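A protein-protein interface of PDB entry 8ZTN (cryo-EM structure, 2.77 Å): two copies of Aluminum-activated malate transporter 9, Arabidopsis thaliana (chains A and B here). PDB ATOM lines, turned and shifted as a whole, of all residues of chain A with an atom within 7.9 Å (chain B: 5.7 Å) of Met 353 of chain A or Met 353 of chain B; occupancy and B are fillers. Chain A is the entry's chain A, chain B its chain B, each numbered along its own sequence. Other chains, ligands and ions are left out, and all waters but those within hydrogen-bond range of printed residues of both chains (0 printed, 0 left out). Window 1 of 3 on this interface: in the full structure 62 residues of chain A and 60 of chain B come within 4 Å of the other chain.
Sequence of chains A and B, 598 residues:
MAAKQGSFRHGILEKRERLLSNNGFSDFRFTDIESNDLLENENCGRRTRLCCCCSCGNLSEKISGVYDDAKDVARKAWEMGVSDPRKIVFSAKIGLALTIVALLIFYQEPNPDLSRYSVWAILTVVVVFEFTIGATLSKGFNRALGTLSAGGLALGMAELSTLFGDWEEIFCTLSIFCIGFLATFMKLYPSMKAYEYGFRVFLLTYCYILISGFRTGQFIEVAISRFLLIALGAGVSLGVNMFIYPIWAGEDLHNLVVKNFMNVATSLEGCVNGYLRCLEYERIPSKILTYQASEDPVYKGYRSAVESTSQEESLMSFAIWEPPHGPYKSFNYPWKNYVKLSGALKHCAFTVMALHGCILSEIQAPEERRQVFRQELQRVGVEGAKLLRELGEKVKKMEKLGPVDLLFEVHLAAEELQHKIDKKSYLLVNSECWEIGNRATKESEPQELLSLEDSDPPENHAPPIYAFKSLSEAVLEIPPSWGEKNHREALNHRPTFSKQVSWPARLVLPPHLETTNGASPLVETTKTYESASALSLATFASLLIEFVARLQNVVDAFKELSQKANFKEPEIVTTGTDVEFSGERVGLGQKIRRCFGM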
ATOM      1  N   SER A 267       9.456 -16.742 -12.018  1.00  0.00           N
ATOM      2  CA  SER A 267       8.434 -17.177 -11.073  1.00  0.00           C
ATOM      3  C   SER A 267       7.405 -16.082 -10.820  1.00  0.00           C
ATOM      4  O   SER A 267       6.199 -16.355 -10.773  1.00  0.00           O
ATOM      5  CB  SER A 267       9.083 -17.617  -9.761  1.00  0.00           C
ATOM      6  OG  SER A 267       9.773 -18.842  -9.926  1.00  0.00           O
ATOM      7  N   CYS A 271       3.434 -16.461 -11.682  1.00  0.00           N
ATOM      8  CA  CYS A 271       2.402 -16.388 -10.651  1.00  0.00           C
ATOM      9  C   CYS A 271       1.367 -15.325 -10.987  1.00  0.00           C
ATOM     10  O   CYS A 271       0.155 -15.557 -10.846  1.00  0.00           O
ATOM     11  CB  CYS A 271       3.033 -16.105  -9.288  1.00  0.00           C
ATOM     12  SG  CYS A 271       3.893 -17.510  -8.549  1.00  0.00           S
ATOM     13  N   VAL A 298       7.009 -21.522 -12.049  1.00  0.00           N
ATOM     14  CA  VAL A 298       6.208 -20.866 -11.024  1.00  0.00           C
ATOM     15  C   VAL A 298       6.583 -21.400  -9.647  1.00  0.00           C
ATOM     16  O   VAL A 298       6.261 -20.797  -8.624  1.00  0.00           O
ATOM     17  CB  VAL A 298       4.706 -21.058 -11.291  1.00  0.00           C
ATOM     18  CG1 VAL A 298       3.880 -20.281 -10.281  1.00  0.00           C
ATOM     19  CG2 VAL A 298       4.365 -20.632 -12.710  1.00  0.00           C
ATOM     20  N   TYR A 299       7.268 -22.539  -9.636  1.00  0.00           N
ATOM     21  CA  TYR A 299       7.695 -23.206  -8.413  1.00  0.00           C
ATOM     22  C   TYR A 299       9.200 -23.415  -8.366  1.00  0.00           C
ATOM     23  O   TYR A 299       9.843 -23.093  -7.356  1.00  0.00           O
ATOM     24  CB  TYR A 299       6.957 -24.550  -8.285  1.00  0.00           C
ATOM     25  CG  TYR A 299       7.075 -25.229  -6.940  1.00  0.00           C
ATOM     26  CD1 TYR A 299       8.168 -26.029  -6.635  1.00  0.00           C
ATOM     27  CD2 TYR A 299       6.090 -25.073  -5.975  1.00  0.00           C
ATOM     28  CE1 TYR A 299       8.271 -26.659  -5.408  1.00  0.00           C
ATOM     29  CE2 TYR A 299       6.188 -25.692  -4.744  1.00  0.00           C
ATOM     30  CZ  TYR A 299       7.281 -26.482  -4.466  1.00  0.00           C
ATOM     31  OH  TYR A 299       7.383 -27.102  -3.242  1.00  0.00           O
ATOM     32  N   TYR A 302      11.587 -19.965  -7.532  1.00  0.00           N
ATOM     33  CA  TYR A 302      11.718 -19.536  -6.145  1.00  0.00           C
ATOM     34  C   TYR A 302      12.221 -20.664  -5.253  1.00  0.00           C
ATOM     35  O   TYR A 302      12.919 -20.401  -4.269  1.00  0.00           O
ATOM     36  CB  TYR A 302      10.392 -18.945  -5.642  1.00  0.00           C
ATOM     37  CG  TYR A 302       9.290 -19.921  -5.275  1.00  0.00           C
ATOM     38  CD1 TYR A 302       9.395 -20.748  -4.162  1.00  0.00           C
ATOM     39  CD2 TYR A 302       8.126 -19.987  -6.027  1.00  0.00           C
ATOM     40  CE1 TYR A 302       8.383 -21.625  -3.826  1.00  0.00           C
ATOM     41  CE2 TYR A 302       7.109 -20.860  -5.698  1.00  0.00           C
ATOM     42  CZ  TYR A 302       7.244 -21.676  -4.597  1.00  0.00           C
ATOM     43  OH  TYR A 302       6.233 -22.548  -4.266  1.00  0.00           O
ATOM     44  N   ARG A 303      11.896 -21.921  -5.574  1.00  0.00           N
ATOM     45  CA  ARG A 303      12.423 -23.021  -4.772  1.00  0.00           C
ATOM     46  C   ARG A 303      13.941 -23.097  -4.871  1.00  0.00           C
ATOM     47  O   ARG A 303      14.624 -23.372  -3.877  1.00  0.00           O
ATOM     48  CB  ARG A 303      11.792 -24.340  -5.211  1.00  0.00           C
ATOM     49  CG  ARG A 303      10.416 -24.587  -4.634  1.00  0.00           C
ATOM     50  CD  ARG A 303      10.437 -24.543  -3.116  1.00  0.00           C
ATOM     51  NE  ARG A 303       9.097 -24.635  -2.551  1.00  0.00           N
ATOM     52  CZ  ARG A 303       8.827 -24.588  -1.254  1.00  0.00           C
ATOM     53  NH1 ARG A 303       9.785 -24.450  -0.353  1.00  0.00           N
ATOM     54  NH2 ARG A 303       7.563 -24.681  -0.852  1.00  0.00           N
ATOM     55  N   VAL A 306      15.498 -20.078  -2.977  1.00  0.00           N
ATOM     56  CA  VAL A 306      15.268 -20.063  -1.537  1.00  0.00           C
ATOM     57  C   VAL A 306      15.909 -21.251  -0.832  1.00  0.00           C
ATOM     58  O   VAL A 306      15.899 -21.303   0.408  1.00  0.00           O
ATOM     59  CB  VAL A 306      13.756 -19.993  -1.232  1.00  0.00           C
ATOM     60  CG1 VAL A 306      13.421 -20.566   0.138  1.00  0.00           C
ATOM     61  CG2 VAL A 306      13.258 -18.559  -1.347  1.00  0.00           C
ATOM     62  N   LYS A 346      16.651 -13.373  -1.649  1.00  0.00           N
ATOM     63  CA  LYS A 346      15.820 -14.418  -1.055  1.00  0.00           C
ATOM     64  C   LYS A 346      14.734 -13.827  -0.162  1.00  0.00           C
ATOM     65  O   LYS A 346      13.642 -14.406  -0.029  1.00  0.00           O
ATOM     66  CB  LYS A 346      16.705 -15.393  -0.279  1.00  0.00           C
ATOM     67  CG  LYS A 346      16.022 -16.120   0.859  1.00  0.00           C
ATOM     68  CD  LYS A 346      17.050 -16.803   1.743  1.00  0.00           C
ATOM     69  CE  LYS A 346      16.395 -17.694   2.780  1.00  0.00           C
ATOM     70  NZ  LYS A 346      17.106 -18.994   2.923  1.00  0.00           N
ATOM     71  N   HIS A 347      15.001 -12.660   0.427  1.00  0.00           N
ATOM     72  CA  HIS A 347      13.970 -12.012   1.233  1.00  0.00           C
ATOM     73  C   HIS A 347      12.740 -11.670   0.389  1.00  0.00           C
ATOM     74  O   HIS A 347      11.604 -11.806   0.855  1.00  0.00           O
ATOM     75  CB  HIS A 347      14.550 -10.765   1.903  1.00  0.00           C
ATOM     76  CG  HIS A 347      13.695 -10.209   3.000  1.00  0.00           C
ATOM     77  ND1 HIS A 347      13.059  -8.990   2.906  1.00  0.00           N
ATOM     78  CD2 HIS A 347      13.376 -10.706   4.218  1.00  0.00           C
ATOM     79  CE1 HIS A 347      12.384  -8.761   4.018  1.00  0.00           C
ATOM     80  NE2 HIS A 347      12.559  -9.788   4.830  1.00  0.00           N
ATOM     81  N   CYS A 348      12.947 -11.213  -0.852  1.00  0.00           N
ATOM     82  CA  CYS A 348      11.843 -11.029  -1.799  1.00  0.00           C
ATOM     83  C   CYS A 348      11.237 -12.362  -2.236  1.00  0.00           C
ATOM     84  O   CYS A 348      10.013 -12.475  -2.435  1.00  0.00           O
ATOM     85  CB  CYS A 348      12.330 -10.245  -3.017  1.00  0.00           C
ATOM     86  SG  CYS A 348      12.250  -8.452  -2.851  1.00  0.00           S
ATOM     87  N   ALA A 349      12.081 -13.375  -2.432  1.00  0.00           N
ATOM     88  CA  ALA A 349      11.554 -14.651  -2.899  1.00  0.00           C
ATOM     89  C   ALA A 349      10.587 -15.268  -1.894  1.00  0.00           C
ATOM     90  O   ALA A 349       9.715 -16.049  -2.287  1.00  0.00           O
ATOM     91  CB  ALA A 349      12.697 -15.620  -3.195  1.00  0.00           C
ATOM     92  N   PHE A 350      10.707 -14.925  -0.610  1.00  0.00           N
ATOM     93  CA  PHE A 350       9.685 -15.351   0.351  1.00  0.00           C
ATOM     94  C   PHE A 350       8.303 -14.788   0.003  1.00  0.00           C
ATOM     95  O   PHE A 350       7.299 -15.515   0.019  1.00  0.00           O
ATOM     96  CB  PHE A 350      10.078 -14.945   1.772  1.00  0.00           C
ATOM     97  CG  PHE A 350      11.215 -15.736   2.339  1.00  0.00           C
ATOM     98  CD1 PHE A 350      11.217 -17.117   2.259  1.00  0.00           C
ATOM     99  CD2 PHE A 350      12.272 -15.107   2.971  1.00  0.00           C
ATOM    100  CE1 PHE A 350      12.256 -17.855   2.785  1.00  0.00           C
ATOM    101  CE2 PHE A 350      13.314 -15.840   3.499  1.00  0.00           C
ATOM    102  CZ  PHE A 350      13.305 -17.215   3.406  1.00  0.00           C
ATOM    103  N   THR A 351       8.227 -13.488  -0.293  1.00  0.00           N
ATOM    104  CA  THR A 351       6.959 -12.908  -0.730  1.00  0.00           C
ATOM    105  C   THR A 351       6.443 -13.598  -1.986  1.00  0.00           C
ATOM    106  O   THR A 351       5.232 -13.799  -2.148  1.00  0.00           O
ATOM    107  CB  THR A 351       7.112 -11.407  -0.969  1.00  0.00           C
ATOM    108  OG1 THR A 351       7.736 -10.802   0.169  1.00  0.00           O
ATOM    109  CG2 THR A 351       5.753 -10.767  -1.187  1.00  0.00           C
ATOM    110  N   VAL A 352       7.349 -13.958  -2.895  1.00  0.00           N
ATOM    111  CA  VAL A 352       6.899 -14.628  -4.115  1.00  0.00           C
ATOM    112  C   VAL A 352       6.313 -16.002  -3.788  1.00  0.00           C
ATOM    113  O   VAL A 352       5.299 -16.421  -4.368  1.00  0.00           O
ATOM    114  CB  VAL A 352       8.048 -14.729  -5.133  1.00  0.00           C
ATOM    115  CG1 VAL A 352       7.552 -15.353  -6.424  1.00  0.00           C
ATOM    116  CG2 VAL A 352       8.631 -13.355  -5.406  1.00  0.00           C
ATOM    117  N   MET A 353       6.942 -16.728  -2.863  1.00  0.00           N
ATOM    118  CA  MET A 353       6.373 -17.988  -2.389  1.00  0.00           C
ATOM    119  C   MET A 353       4.988 -17.791  -1.785  1.00  0.00           C
ATOM    120  O   MET A 353       4.097 -18.625  -1.975  1.00  0.00           O
ATOM    121  CB  MET A 353       7.308 -18.636  -1.370  1.00  0.00           C
ATOM    122  CG  MET A 353       6.967 -20.080  -1.058  1.00  0.00           C
ATOM    123  SD  MET A 353       7.246 -20.509   0.669  1.00  0.00           S
ATOM    124  CE  MET A 353       9.005 -20.843   0.657  1.00  0.00           C
ATOM    125  N   ALA A 354       4.785 -16.699  -1.045  1.00  0.00           N
ATOM    126  CA  ALA A 354       3.454 -16.453  -0.487  1.00  0.00           C
ATOM    127  C   ALA A 354       2.430 -16.140  -1.576  1.00  0.00           C
ATOM    128  O   ALA A 354       1.260 -16.538  -1.470  1.00  0.00           O
ATOM    129  CB  ALA A 354       3.510 -15.316   0.532  1.00  0.00           C
ATOM    130  N   LEU A 355       2.860 -15.480  -2.654  1.00  0.00           N
ATOM    131  CA  LEU A 355       1.929 -15.222  -3.749  1.00  0.00           C
ATOM    132  C   LEU A 355       1.583 -16.503  -4.492  1.00  0.00           C
ATOM    133  O   LEU A 355       0.469 -16.637  -5.010  1.00  0.00           O
ATOM    134  CB  LEU A 355       2.509 -14.194  -4.720  1.00  0.00           C
ATOM    135  CG  LEU A 355       2.441 -12.720  -4.320  1.00  0.00           C
ATOM    136  CD1 LEU A 355       3.426 -11.898  -5.133  1.00  0.00           C
ATOM    137  CD2 LEU A 355       1.029 -12.194  -4.498  1.00  0.00           C
ATOM    138  N   HIS A 356       2.517 -17.455  -4.551  1.00  0.00           N
ATOM    139  CA  HIS A 356       2.177 -18.760  -5.113  1.00  0.00           C
ATOM    140  C   HIS A 356       1.245 -19.537  -4.190  1.00  0.00           C
ATOM    141  O   HIS A 356       0.326 -20.220  -4.655  1.00  0.00           O
ATOM    142  CB  HIS A 356       3.442 -19.571  -5.382  1.00  0.00           C
ATOM    143  CG  HIS A 356       3.187 -20.860  -6.100  1.00  0.00           C
ATOM    144  ND1 HIS A 356       3.846 -22.029  -5.788  1.00  0.00           N
ATOM    145  CD2 HIS A 356       2.339 -21.164  -7.110  1.00  0.00           C
ATOM    146  CE1 HIS A 356       3.417 -22.997  -6.577  1.00  0.00           C
ATOM    147  NE2 HIS A 356       2.504 -22.499  -7.389  1.00  0.00           N
ATOM    148  N   GLY A 357       1.470 -19.444  -2.880  1.00  0.00           N
ATOM    149  CA  GLY A 357       0.557 -20.059  -1.928  1.00  0.00           C
ATOM    150  C   GLY A 357      -0.866 -19.550  -2.052  1.00  0.00           C
ATOM    151  O   GLY A 357      -1.824 -20.305  -1.863  1.00  0.00           O
ATOM    152  N   CYS A 358      -1.028 -18.263  -2.360  1.00  0.00           N
ATOM    153  CA  CYS A 358      -2.377 -17.720  -2.524  1.00  0.00           C
ATOM    154  C   CYS A 358      -3.165 -18.426  -3.627  1.00  0.00           C
ATOM    155  O   CYS A 358      -4.394 -18.516  -3.544  1.00  0.00           O
ATOM    156  CB  CYS A 358      -2.315 -16.220  -2.814  1.00  0.00           C
ATOM    157  SG  CYS A 358      -2.570 -15.164  -1.372  1.00  0.00           S
ATOM    158  N   ILE A 359      -2.489 -18.925  -4.666  1.00  0.00           N
ATOM    159  CA  ILE A 359      -3.195 -19.628  -5.738  1.00  0.00           C
ATOM    160  C   ILE A 359      -3.703 -20.997  -5.294  1.00  0.00           C
ATOM    161  O   ILE A 359      -4.720 -21.481  -5.806  1.00  0.00           O
ATOM    162  CB  ILE A 359      -2.298 -19.751  -6.985  1.00  0.00           C
ATOM    163  CG1 ILE A 359      -2.105 -18.386  -7.647  1.00  0.00           C
ATOM    164  CG2 ILE A 359      -2.896 -20.734  -7.976  1.00  0.00           C
ATOM    165  CD1 ILE A 359      -0.715 -18.166  -8.190  1.00  0.00           C
ATOM    166  N   LEU A 360      -3.021 -21.649  -4.355  1.00  0.00           N
ATOM    167  CA  LEU A 360      -3.417 -22.974  -3.894  1.00  0.00           C
ATOM    168  C   LEU A 360      -4.401 -22.948  -2.732  1.00  0.00           C
ATOM    169  O   LEU A 360      -4.757 -24.015  -2.220  1.00  0.00           O
ATOM    170  CB  LEU A 360      -2.181 -23.788  -3.492  1.00  0.00           C
ATOM    171  CG  LEU A 360      -1.013 -23.811  -4.479  1.00  0.00           C
ATOM    172  CD1 LEU A 360       0.270 -24.233  -3.780  1.00  0.00           C
ATOM    173  CD2 LEU A 360      -1.319 -24.734  -5.645  1.00  0.00           C
ATOM    174  N   LEU A 543       0.067  -8.418  -0.911  1.00  0.00           N
ATOM    175  CA  LEU A 543       1.322  -9.146  -1.055  1.00  0.00           C
ATOM    176  C   LEU A 543       2.144  -8.593  -2.213  1.00  0.00           C
ATOM    177  O   LEU A 543       3.360  -8.404  -2.089  1.00  0.00           O
ATOM    178  CB  LEU A 543       1.047 -10.638  -1.243  1.00  0.00           C
ATOM    179  CG  LEU A 543       0.615 -11.399   0.011  1.00  0.00           C
ATOM    180  CD1 LEU A 543       0.240 -12.831  -0.328  1.00  0.00           C
ATOM    181  CD2 LEU A 543       1.709 -11.361   1.065  1.00  0.00           C
ATOM    182  N   PHE A 547       5.893  -6.945  -1.879  1.00  0.00           N
ATOM    183  CA  PHE A 547       7.008  -7.285  -2.762  1.00  0.00           C
ATOM    184  C   PHE A 547       7.664  -6.027  -3.326  1.00  0.00           C
ATOM    185  O   PHE A 547       8.897  -5.871  -3.298  1.00  0.00           O
ATOM    186  CB  PHE A 547       6.508  -8.194  -3.887  1.00  0.00           C
ATOM    187  CG  PHE A 547       7.492  -8.384  -5.008  1.00  0.00           C
ATOM    188  CD1 PHE A 547       8.485  -9.343  -4.917  1.00  0.00           C
ATOM    189  CD2 PHE A 547       7.419  -7.612  -6.153  1.00  0.00           C
ATOM    190  CE1 PHE A 547       9.389  -9.524  -5.944  1.00  0.00           C
ATOM    191  CE2 PHE A 547       8.320  -7.787  -7.181  1.00  0.00           C
ATOM    192  CZ  PHE A 547       9.306  -8.745  -7.077  1.00  0.00           C
ATOM    193  N   TYR B 302       8.440 -24.144  12.751  1.00  0.00           N
ATOM    194  CA  TYR B 302       8.027 -24.351  11.369  1.00  0.00           C
ATOM    195  C   TYR B 302       9.222 -24.605  10.459  1.00  0.00           C
ATOM    196  O   TYR B 302       9.093 -25.335   9.470  1.00  0.00           O
ATOM    197  CB  TYR B 302       7.175 -23.172  10.878  1.00  0.00           C
ATOM    198  CG  TYR B 302       7.907 -21.891  10.534  1.00  0.00           C
ATOM    199  CD1 TYR B 302       8.669 -21.786   9.378  1.00  0.00           C
ATOM    200  CD2 TYR B 302       7.802 -20.774  11.350  1.00  0.00           C
ATOM    201  CE1 TYR B 302       9.326 -20.614   9.060  1.00  0.00           C
ATOM    202  CE2 TYR B 302       8.454 -19.598  11.038  1.00  0.00           C
ATOM    203  CZ  TYR B 302       9.214 -19.524   9.892  1.00  0.00           C
ATOM    204  OH  TYR B 302       9.864 -18.353   9.578  1.00  0.00           O
ATOM    205  N   ARG B 303      10.389 -24.031  10.766  1.00  0.00           N
ATOM    206  CA  ARG B 303      11.562 -24.313   9.945  1.00  0.00           C
ATOM    207  C   ARG B 303      11.948 -25.785  10.025  1.00  0.00           C
ATOM    208  O   ARG B 303      12.340 -26.389   9.019  1.00  0.00           O
ATOM    209  CB  ARG B 303      12.731 -23.431  10.377  1.00  0.00           C
ATOM    210  CG  ARG B 303      12.685 -22.028   9.816  1.00  0.00           C
ATOM    211  CD  ARG B 303      12.624 -22.041   8.299  1.00  0.00           C
ATOM    212  NE  ARG B 303      12.436 -20.704   7.752  1.00  0.00           N
ATOM    213  CZ  ARG B 303      12.317 -20.434   6.459  1.00  0.00           C
ATOM    214  NH1 ARG B 303      12.366 -21.390   5.546  1.00  0.00           N
ATOM    215  NH2 ARG B 303      12.146 -19.173   6.072  1.00  0.00           N
ATOM    216  N   VAL B 306       9.270 -27.913   8.156  1.00  0.00           N
ATOM    217  CA  VAL B 306       9.187 -27.681   6.719  1.00  0.00           C
ATOM    218  C   VAL B 306      10.469 -28.061   5.992  1.00  0.00           C
ATOM    219  O   VAL B 306      10.499 -28.035   4.752  1.00  0.00           O
ATOM    220  CB  VAL B 306       8.806 -26.214   6.428  1.00  0.00           C
ATOM    221  CG1 VAL B 306       9.301 -25.751   5.066  1.00  0.00           C
ATOM    222  CG2 VAL B 306       7.299 -26.024   6.541  1.00  0.00           C
ATOM    223  N   ALA B 349       1.814 -26.007   7.766  1.00  0.00           N
ATOM    224  CA  ALA B 349       2.890 -25.165   8.293  1.00  0.00           C
ATOM    225  C   ALA B 349       3.301 -24.048   7.335  1.00  0.00           C
ATOM    226  O   ALA B 349       3.870 -23.037   7.777  1.00  0.00           O
ATOM    227  CB  ALA B 349       4.106 -26.024   8.637  1.00  0.00           C
ATOM    228  N   PHE B 350       3.035 -24.202   6.037  1.00  0.00           N
ATOM    229  CA  PHE B 350       3.290 -23.085   5.122  1.00  0.00           C
ATOM    230  C   PHE B 350       2.508 -21.827   5.517  1.00  0.00           C
ATOM    231  O   PHE B 350       3.050 -20.712   5.478  1.00  0.00           O
ATOM    232  CB  PHE B 350       2.957 -23.480   3.683  1.00  0.00           C
ATOM    233  CG  PHE B 350       3.931 -24.444   3.075  1.00  0.00           C
ATOM    234  CD1 PHE B 350       5.293 -24.220   3.167  1.00  0.00           C
ATOM    235  CD2 PHE B 350       3.488 -25.565   2.396  1.00  0.00           C
ATOM    236  CE1 PHE B 350       6.195 -25.101   2.604  1.00  0.00           C
ATOM    237  CE2 PHE B 350       4.385 -26.449   1.831  1.00  0.00           C
ATOM    238  CZ  PHE B 350       5.740 -26.216   1.935  1.00  0.00           C
ATOM    239  N   THR B 351       1.229 -21.976   5.868  1.00  0.00           N
ATOM    240  CA  THR B 351       0.445 -20.828   6.323  1.00  0.00           C
ATOM    241  C   THR B 351       1.078 -20.153   7.537  1.00  0.00           C
ATOM    242  O   THR B 351       1.043 -18.924   7.662  1.00  0.00           O
ATOM    243  CB  THR B 351      -0.988 -21.254   6.635  1.00  0.00           C
ATOM    244  OG1 THR B 351      -1.518 -21.999   5.533  1.00  0.00           O
ATOM    245  CG2 THR B 351      -1.860 -20.034   6.876  1.00  0.00           C
ATOM    246  N   VAL B 352       1.648 -20.939   8.451  1.00  0.00           N
ATOM    247  CA  VAL B 352       2.278 -20.354   9.630  1.00  0.00           C
ATOM    248  C   VAL B 352       3.528 -19.580   9.235  1.00  0.00           C
ATOM    249  O   VAL B 352       3.821 -18.513   9.793  1.00  0.00           O
ATOM    250  CB  VAL B 352       2.592 -21.446  10.669  1.00  0.00           C
ATOM    251  CG1 VAL B 352       3.161 -20.824  11.931  1.00  0.00           C
ATOM    252  CG2 VAL B 352       1.342 -22.245  10.992  1.00  0.00           C
ATOM    253  N   MET B 353       4.297 -20.109   8.284  1.00  0.00           N
ATOM    254  CA  MET B 353       5.422 -19.340   7.758  1.00  0.00           C
ATOM    255  C   MET B 353       4.960 -18.012   7.162  1.00  0.00           C
ATOM    256  O   MET B 353       5.617 -16.979   7.340  1.00  0.00           O
ATOM    257  CB  MET B 353       6.181 -20.156   6.714  1.00  0.00           C
ATOM    258  CG  MET B 353       7.486 -19.514   6.271  1.00  0.00           C
ATOM    259  SD  MET B 353       7.805 -19.694   4.508  1.00  0.00           S
ATOM    260  CE  MET B 353       8.488 -21.347   4.456  1.00  0.00           C
ATOM    261  N   ALA B 354       3.818 -18.012   6.472  1.00  0.00           N
ATOM    262  CA  ALA B 354       3.303 -16.755   5.926  1.00  0.00           C
ATOM    263  C   ALA B 354       2.827 -15.802   7.021  1.00  0.00           C
ATOM    264  O   ALA B 354       2.981 -14.578   6.895  1.00  0.00           O
ATOM    265  CB  ALA B 354       2.170 -17.034   4.939  1.00  0.00           C
ATOM    266  N   LEU B 355       2.297 -16.338   8.122  1.00  0.00           N
ATOM    267  CA  LEU B 355       1.884 -15.468   9.219  1.00  0.00           C
ATOM    268  C   LEU B 355       3.087 -14.876   9.937  1.00  0.00           C
ATOM    269  O   LEU B 355       3.011 -13.754  10.451  1.00  0.00           O
ATOM    270  CB  LEU B 355       1.006 -16.233  10.210  1.00  0.00           C
ATOM    271  CG  LEU B 355      -0.458 -16.462   9.837  1.00  0.00           C
ATOM    272  CD1 LEU B 355      -1.049 -17.587  10.667  1.00  0.00           C
ATOM    273  CD2 LEU B 355      -1.257 -15.185  10.018  1.00  0.00           C
ATOM    274  N   HIS B 356       4.199 -15.608   9.983  1.00  0.00           N
ATOM    275  CA  HIS B 356       5.428 -15.031  10.518  1.00  0.00           C
ATOM    276  C   HIS B 356       5.993 -13.974   9.578  1.00  0.00           C
ATOM    277  O   HIS B 356       6.497 -12.939  10.028  1.00  0.00           O
ATOM    278  CB  HIS B 356       6.463 -16.126  10.768  1.00  0.00           C
ATOM    279  CG  HIS B 356       7.697 -15.639  11.459  1.00  0.00           C
ATOM    280  ND1 HIS B 356       8.961 -16.075  11.122  1.00  0.00           N
ATOM    281  CD2 HIS B 356       7.863 -14.752  12.470  1.00  0.00           C
ATOM    282  CE1 HIS B 356       9.851 -15.477  11.894  1.00  0.00           C
ATOM    283  NE2 HIS B 356       9.211 -14.671  12.721  1.00  0.00           N
ATOM    284  N   GLY B 357       5.916 -14.218   8.269  1.00  0.00           N
ATOM    285  CA  GLY B 357       6.300 -13.193   7.310  1.00  0.00           C
ATOM    286  C   GLY B 357       5.504 -11.910   7.459  1.00  0.00           C
ATOM    287  O   GLY B 357       6.035 -10.814   7.268  1.00  0.00           O
ATOM    288  N   CYS B 358       4.218 -12.028   7.791  1.00  0.00           N
ATOM    289  CA  CYS B 358       3.402 -10.831   7.997  1.00  0.00           C
ATOM    290  C   CYS B 358       3.944  -9.938   9.112  1.00  0.00           C
ATOM    291  O   CYS B 358       3.772  -8.716   9.060  1.00  0.00           O
ATOM    292  CB  CYS B 358       1.955 -11.220   8.304  1.00  0.00           C
ATOM    293  SG  CYS B 358       0.832 -11.122   6.895  1.00  0.00           S
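The side-chain hydroxyl of Tyr 299 of chain A lies within hydrogen-bond range of the guanidinium group of Arg 303 of chain A (3.1 Å).
Arg 303 of chain A touches Phe 350 of chain B (NH2 to CZ, 3.7 Å).
Phe 350 of chain A touches Arg 303 of chain B (CZ to NH2, 3.5 Å).
CE of Met 353 of chain B touches CE of Met 353 of chain A, at 3.9 Å.
Met 353 of chain A touches just one residue of chain B: Met 353.
Met 353 of chain B touches just one residue of chain A: Met 353 (3.9 Å).
Printed residues of chain B within 4 Å of Phe 350 of chain A: Arg 303 (3.5 Å).
Printed residues of chain A within 4 Å of Arg 303 of chain B: Phe 350.
Printed residues of chain B within 4 Å of Arg 303 of chain A: Phe 350.
Of the printed residues of chain A, Phe 350 of chain B touches Arg 303 (3.7 Å).
The nearest residue of chain B that does not touch Met 353 of chain A is Phe 350 of chain B (4.9 Å).
The nearest residue of chain A that does not touch Met 353 of chain B is Phe 350 of chain A (4.8 Å).
Of the 24 printed residues of chain A, 3 touch a printed residue of chain B.
Of the 13 printed residues of chain B, 3 touch a printed residue of chain A.
Printed residues of chain B that touch a printed residue of chain A: Arg 303, Phe 350 and Met 353.
Hydrophobic or aromatic side chains of chain B that line the printed part of chain A: Phe 350 and Met 353.
Among the printed residues, no Asp or Glu carboxylate lies within 4 Å of a Lys or Arg side-chain nitrogen of the other chain.
Arg 303 of chain A touches Phe 350 of chain B, and with the chains exchanged Phe 350 of chain A touches Arg 303 of chain B.
Met 353 of chain A touches its own counterpart, Met 353 of chain B.
Positions printed for both chains: 302, 303, 306, 349, 350, 351, 352, 353, 354, 355, 356, 357 and 358.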
